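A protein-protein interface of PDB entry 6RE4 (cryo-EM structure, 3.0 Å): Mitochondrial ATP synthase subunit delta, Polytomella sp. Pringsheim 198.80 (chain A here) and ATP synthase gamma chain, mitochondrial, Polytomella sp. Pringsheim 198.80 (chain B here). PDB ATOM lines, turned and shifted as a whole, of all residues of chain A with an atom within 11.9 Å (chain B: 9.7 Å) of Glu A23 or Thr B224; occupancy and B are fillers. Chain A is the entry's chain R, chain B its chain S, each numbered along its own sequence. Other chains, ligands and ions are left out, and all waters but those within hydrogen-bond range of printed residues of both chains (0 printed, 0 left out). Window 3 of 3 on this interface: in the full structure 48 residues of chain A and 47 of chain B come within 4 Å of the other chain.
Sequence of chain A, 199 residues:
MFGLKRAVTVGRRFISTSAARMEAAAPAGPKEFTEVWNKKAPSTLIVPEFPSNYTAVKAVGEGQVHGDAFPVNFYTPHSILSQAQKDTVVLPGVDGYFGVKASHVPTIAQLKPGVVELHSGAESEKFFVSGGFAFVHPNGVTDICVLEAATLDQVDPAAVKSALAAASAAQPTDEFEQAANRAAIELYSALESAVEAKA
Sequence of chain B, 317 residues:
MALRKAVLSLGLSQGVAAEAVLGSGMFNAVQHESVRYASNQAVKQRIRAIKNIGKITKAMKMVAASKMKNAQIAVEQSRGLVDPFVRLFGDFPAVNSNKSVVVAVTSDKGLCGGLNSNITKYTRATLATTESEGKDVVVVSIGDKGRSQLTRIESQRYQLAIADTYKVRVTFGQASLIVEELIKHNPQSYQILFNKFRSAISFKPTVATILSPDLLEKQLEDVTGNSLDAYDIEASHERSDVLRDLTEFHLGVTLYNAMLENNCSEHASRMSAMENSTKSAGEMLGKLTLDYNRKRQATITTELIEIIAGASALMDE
The backbone NH (N) of Ala A24 lies close to the backbone carbonyl oxygen (O) of Asp B222.
The side-chain carboxylate of Glu A23 is in hydrogen-bond range of the backbone NH of Gly B225.
The backbone carbonyl oxygen (O) of Glu A23 lies close to the backbone carbonyl oxygen (O) of Asp B222.
The backbone carbonyl oxygen (O) of Gln B219 lies close to the backbone carbonyl oxygen (O) of Glu A23, 3.4 Å away.
The side-chain amide nitrogen (ND2) of Asn B226 sits at hydrogen-bond distance from the side-chain carboxylate (OD2) of Asp B222.
Glu A23 touches Thr B224 (OE2 to CA, 3.3 Å).
Ala A26 touches Leu B220 (O to CD1, 3.3 Å).
Of chain B, only Gln B219 (3.4 Å), Asp B222 (3.0 Å), Thr B224 (3.3 Å) and Gly B225 (3.3 Å) come within 4 Å of Glu A23.
Of chain B, only Asp B222 (3.3 Å) comes within 4 Å of Ala A24.
Of the printed residues of chain B, Ala A26 touches Leu B220 (3.3 Å).
Printed residues of chain A within 4 Å of Gln B219: Glu A23 (3.4 Å).
Printed residues of chain A within 4 Å of Leu B220: Ala A26 (3.3 Å).
Asp B222 touches just these residues of chain A: Glu A23 (3.0 Å) and Ala A24 (3.3 Å).
No residue of chain A comes within 4 Å of Val B223.
Of chain A, only Glu A23 comes within 4 Å of Thr B224.
Of chain A, only Glu A23 comes within 4 Å of Gly B225.
Leu B228 touches none of the printed residues of chain A.
The nearest residue of chain B that does not touch Glu A23 is Val B223 (4.9 Å).
Of the 14 printed residues of chain B, 5 touch a printed residue of chain A.
Printed residues of chain B that touch a printed residue of chain A: Gln B219, Leu B220, Asp B222, Thr B224 and Gly B225.
Along chain B the printed residues that touch a printed residue of chain A span positions 219 to 225.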
ATOM      1  N   GLU A  23     -34.048  -5.714  -0.039  1.00  0.00           N
ATOM      2  CA  GLU A  23     -32.726  -5.456   0.513  1.00  0.00           C
ATOM      3  C   GLU A  23     -32.241  -6.567   1.449  1.00  0.00           C
ATOM      4  O   GLU A  23     -31.081  -6.970   1.386  1.00  0.00           O
ATOM      5  CB  GLU A  23     -32.713  -4.095   1.220  1.00  0.00           C
ATOM      6  CG  GLU A  23     -33.816  -3.874   2.243  1.00  0.00           C
ATOM      7  CD  GLU A  23     -33.673  -2.560   2.976  1.00  0.00           C
ATOM      8  OE1 GLU A  23     -32.637  -1.887   2.804  1.00  0.00           O
ATOM      9  OE2 GLU A  23     -34.616  -2.180   3.695  1.00  0.00           O
ATOM     10  N   ALA A  24     -33.126  -7.080   2.300  1.00  0.00           N
ATOM     11  CA  ALA A  24     -32.811  -8.173   3.211  1.00  0.00           C
ATOM     12  C   ALA A  24     -33.576  -9.432   2.819  1.00  0.00           C
ATOM     13  O   ALA A  24     -33.925 -10.257   3.665  1.00  0.00           O
ATOM     14  CB  ALA A  24     -33.119  -7.785   4.653  1.00  0.00           C
ATOM     15  N   ALA A  25     -33.828  -9.593   1.521  1.00  0.00           N
ATOM     16  CA  ALA A  25     -34.808 -10.544   1.020  1.00  0.00           C
ATOM     17  C   ALA A  25     -34.248 -11.945   0.829  1.00  0.00           C
ATOM     18  O   ALA A  25     -34.939 -12.805   0.270  1.00  0.00           O
ATOM     19  CB  ALA A  25     -35.402 -10.039  -0.297  1.00  0.00           C
ATOM     20  N   ALA A  26     -33.022 -12.202   1.278  1.00  0.00           N
ATOM     21  CA  ALA A  26     -32.445 -13.543   1.205  1.00  0.00           C
ATOM     22  C   ALA A  26     -31.696 -13.824   2.491  1.00  0.00           C
ATOM     23  O   ALA A  26     -30.473 -13.647   2.567  1.00  0.00           O
ATOM     24  CB  ALA A  26     -31.524 -13.693  -0.004  1.00  0.00           C
ATOM     25  N   PRO A  27     -32.393 -14.268   3.532  1.00  0.00           N
ATOM     26  CA  PRO A  27     -31.691 -14.645   4.774  1.00  0.00           C
ATOM     27  C   PRO A  27     -30.897 -15.939   4.624  1.00  0.00           C
ATOM     28  O   PRO A  27     -31.306 -17.025   5.025  1.00  0.00           O
ATOM     29  CB  PRO A  27     -32.837 -14.791   5.779  1.00  0.00           C
ATOM     30  CG  PRO A  27     -34.001 -14.104   5.162  1.00  0.00           C
ATOM     31  CD  PRO A  27     -33.850 -14.314   3.703  1.00  0.00           C
ATOM     32  N   ALA A  28     -29.719 -15.809   4.018  1.00  0.00           N
ATOM     33  CA  ALA A  28     -28.768 -16.903   3.949  1.00  0.00           C
ATOM     34  C   ALA A  28     -28.158 -17.153   5.323  1.00  0.00           C
ATOM     35  O   ALA A  28     -28.317 -16.368   6.261  1.00  0.00           O
ATOM     36  CB  ALA A  28     -27.663 -16.590   2.944  1.00  0.00           C
ATOM     37  N   LEU B 216     -22.465  -9.273  -4.840  1.00  0.00           N
ATOM     38  CA  LEU B 216     -23.331  -9.974  -3.897  1.00  0.00           C
ATOM     39  C   LEU B 216     -23.065  -9.645  -2.440  1.00  0.00           C
ATOM     40  O   LEU B 216     -23.980  -9.795  -1.625  1.00  0.00           O
ATOM     41  CB  LEU B 216     -23.201 -11.487  -4.085  1.00  0.00           C
ATOM     42  CG  LEU B 216     -24.423 -12.303  -3.683  1.00  0.00           C
ATOM     43  CD1 LEU B 216     -25.608 -11.936  -4.543  1.00  0.00           C
ATOM     44  CD2 LEU B 216     -24.108 -13.760  -3.788  1.00  0.00           C
ATOM     45  N   GLU B 217     -21.867  -9.195  -2.074  1.00  0.00           N
ATOM     46  CA  GLU B 217     -21.562  -8.979  -0.668  1.00  0.00           C
ATOM     47  C   GLU B 217     -22.277  -7.747  -0.141  1.00  0.00           C
ATOM     48  O   GLU B 217     -22.857  -7.779   0.945  1.00  0.00           O
ATOM     49  CB  GLU B 217     -20.050  -8.867  -0.477  1.00  0.00           C
ATOM     50  CG  GLU B 217     -19.617  -8.355   0.863  1.00  0.00           C
ATOM     51  CD  GLU B 217     -19.987  -9.287   1.979  1.00  0.00           C
ATOM     52  OE1 GLU B 217     -19.990 -10.514   1.757  1.00  0.00           O
ATOM     53  OE2 GLU B 217     -20.270  -8.794   3.086  1.00  0.00           O
ATOM     54  N   LYS B 218     -22.286  -6.665  -0.920  1.00  0.00           N
ATOM     55  CA  LYS B 218     -23.047  -5.486  -0.523  1.00  0.00           C
ATOM     56  C   LYS B 218     -24.546  -5.724  -0.578  1.00  0.00           C
ATOM     57  O   LYS B 218     -25.295  -5.086   0.164  1.00  0.00           O
ATOM     58  CB  LYS B 218     -22.673  -4.296  -1.398  1.00  0.00           C
ATOM     59  CG  LYS B 218     -21.297  -3.747  -1.112  1.00  0.00           C
ATOM     60  CD  LYS B 218     -21.259  -3.166   0.278  1.00  0.00           C
ATOM     61  CE  LYS B 218     -22.073  -1.900   0.345  1.00  0.00           C
ATOM     62  NZ  LYS B 218     -21.454  -0.823  -0.475  1.00  0.00           N
ATOM     63  N   GLN B 219     -25.008  -6.633  -1.432  1.00  0.00           N
ATOM     64  CA  GLN B 219     -26.437  -6.906  -1.473  1.00  0.00           C
ATOM     65  C   GLN B 219     -26.887  -7.789  -0.321  1.00  0.00           C
ATOM     66  O   GLN B 219     -28.010  -7.630   0.165  1.00  0.00           O
ATOM     67  CB  GLN B 219     -26.815  -7.544  -2.806  1.00  0.00           C
ATOM     68  CG  GLN B 219     -26.726  -6.575  -3.971  1.00  0.00           C
ATOM     69  CD  GLN B 219     -27.137  -7.198  -5.283  1.00  0.00           C
ATOM     70  OE1 GLN B 219     -27.806  -8.229  -5.310  1.00  0.00           O
ATOM     71  NE2 GLN B 219     -26.732  -6.577  -6.380  1.00  0.00           N
ATOM     72  N   LEU B 220     -26.045  -8.709   0.137  1.00  0.00           N
ATOM     73  CA  LEU B 220     -26.444  -9.579   1.236  1.00  0.00           C
ATOM     74  C   LEU B 220     -26.297  -8.933   2.601  1.00  0.00           C
ATOM     75  O   LEU B 220     -26.702  -9.540   3.595  1.00  0.00           O
ATOM     76  CB  LEU B 220     -25.648 -10.884   1.211  1.00  0.00           C
ATOM     77  CG  LEU B 220     -26.382 -12.145   0.749  1.00  0.00           C
ATOM     78  CD1 LEU B 220     -27.441 -12.526   1.764  1.00  0.00           C
ATOM     79  CD2 LEU B 220     -27.008 -11.972  -0.613  1.00  0.00           C
ATOM     80  N   GLU B 221     -25.736  -7.733   2.685  1.00  0.00           N
ATOM     81  CA  GLU B 221     -25.580  -7.071   3.970  1.00  0.00           C
ATOM     82  C   GLU B 221     -26.661  -6.046   4.251  1.00  0.00           C
ATOM     83  O   GLU B 221     -26.704  -5.516   5.362  1.00  0.00           O
ATOM     84  CB  GLU B 221     -24.220  -6.380   4.057  1.00  0.00           C
ATOM     85  CG  GLU B 221     -23.039  -7.317   4.113  1.00  0.00           C
ATOM     86  CD  GLU B 221     -22.958  -8.087   5.390  1.00  0.00           C
ATOM     87  OE1 GLU B 221     -23.470  -7.607   6.417  1.00  0.00           O
ATOM     88  OE2 GLU B 221     -22.369  -9.177   5.374  1.00  0.00           O
ATOM     89  N   ASP B 222     -27.524  -5.755   3.281  1.00  0.00           N
ATOM     90  CA  ASP B 222     -28.509  -4.684   3.404  1.00  0.00           C
ATOM     91  C   ASP B 222     -29.572  -5.120   4.396  1.00  0.00           C
ATOM     92  O   ASP B 222     -30.480  -5.878   4.067  1.00  0.00           O
ATOM     93  CB  ASP B 222     -29.134  -4.364   2.053  1.00  0.00           C
ATOM     94  CG  ASP B 222     -28.203  -3.608   1.133  1.00  0.00           C
ATOM     95  OD1 ASP B 222     -28.047  -4.030  -0.027  1.00  0.00           O
ATOM     96  OD2 ASP B 222     -27.629  -2.589   1.561  1.00  0.00           O
ATOM     97  N   VAL B 223     -29.444  -4.660   5.640  1.00  0.00           N
ATOM     98  CA  VAL B 223     -30.458  -4.944   6.648  1.00  0.00           C
ATOM     99  C   VAL B 223     -31.137  -3.651   7.097  1.00  0.00           C
ATOM    100  O   VAL B 223     -30.761  -3.045   8.108  1.00  0.00           O
ATOM    101  CB  VAL B 223     -29.840  -5.741   7.817  1.00  0.00           C
ATOM    102  CG1 VAL B 223     -29.721  -7.205   7.425  1.00  0.00           C
ATOM    103  CG2 VAL B 223     -28.438  -5.228   8.172  1.00  0.00           C
ATOM    104  N   THR B 224     -32.204  -3.277   6.377  1.00  0.00           N
ATOM    105  CA  THR B 224     -32.907  -1.982   6.472  1.00  0.00           C
ATOM    106  C   THR B 224     -31.934  -0.799   6.482  1.00  0.00           C
ATOM    107  O   THR B 224     -31.995   0.097   7.325  1.00  0.00           O
ATOM    108  CB  THR B 224     -33.845  -1.944   7.683  1.00  0.00           C
ATOM    109  OG1 THR B 224     -33.085  -2.031   8.894  1.00  0.00           O
ATOM    110  CG2 THR B 224     -34.840  -3.088   7.614  1.00  0.00           C
ATOM    111  N   GLY B 225     -31.053  -0.796   5.489  1.00  0.00           N
ATOM    112  CA  GLY B 225     -29.870   0.044   5.501  1.00  0.00           C
ATOM    113  C   GLY B 225     -28.669  -0.792   5.109  1.00  0.00           C
ATOM    114  O   GLY B 225     -28.670  -1.391   4.031  1.00  0.00           O
ATOM    115  N   ASN B 226     -27.656  -0.874   5.967  1.00  0.00           N
ATOM    116  CA  ASN B 226     -26.549  -1.790   5.730  1.00  0.00           C
ATOM    117  C   ASN B 226     -25.887  -2.130   7.055  1.00  0.00           C
ATOM    118  O   ASN B 226     -25.904  -1.331   7.991  1.00  0.00           O
ATOM    119  CB  ASN B 226     -25.517  -1.206   4.762  1.00  0.00           C
ATOM    120  CG  ASN B 226     -24.686  -2.269   4.088  1.00  0.00           C
ATOM    121  OD1 ASN B 226     -24.142  -3.150   4.743  1.00  0.00           O
ATOM    122  ND2 ASN B 226     -24.590  -2.198   2.769  1.00  0.00           N
ATOM    123  N   SER B 227     -25.308  -3.322   7.119  1.00  0.00           N
ATOM    124  CA  SER B 227     -24.520  -3.756   8.260  1.00  0.00           C
ATOM    125  C   SER B 227     -23.061  -3.391   8.125  1.00  0.00           C
ATOM    126  O   SER B 227     -22.285  -3.627   9.053  1.00  0.00           O
ATOM    127  CB  SER B 227     -24.635  -5.269   8.437  1.00  0.00           C
ATOM    128  OG  SER B 227     -23.773  -5.715   9.462  1.00  0.00           O
ATOM    129  N   LEU B 228     -22.670  -2.840   6.987  1.00  0.00           N
ATOM    130  CA  LEU B 228     -21.291  -2.487   6.725  1.00  0.00           C
ATOM    131  C   LEU B 228     -21.049  -0.995   6.854  1.00  0.00           C
ATOM    132  O   LEU B 228     -19.895  -0.563   6.848  1.00  0.00           O
ATOM    133  CB  LEU B 228     -20.903  -2.967   5.327  1.00  0.00           C
ATOM    134  CG  LEU B 228     -19.449  -3.214   4.978  1.00  0.00           C
ATOM    135  CD1 LEU B 228     -18.926  -4.325   5.849  1.00  0.00           C
ATOM    136  CD2 LEU B 228     -19.381  -3.608   3.536  1.00  0.00           C
ATOM    137  N   ASP B 229     -22.108  -0.201   6.982  1.00  0.00           N
ATOM    138  CA  ASP B 229     -21.993   1.238   7.153  1.00  0.00           C
ATOM    139  C   ASP B 229     -21.461   1.641   8.517  1.00  0.00           C
ATOM    140  O   ASP B 229     -21.133   2.814   8.710  1.00  0.00           O
ATOM    141  CB  ASP B 229     -23.349   1.900   6.947  1.00  0.00           C
ATOM    142  CG  ASP B 229     -23.785   1.898   5.513  1.00  0.00           C
ATOM    143  OD1 ASP B 229     -22.911   1.807   4.629  1.00  0.00           O
ATOM    144  OD2 ASP B 229     -25.000   2.009   5.266  1.00  0.00           O
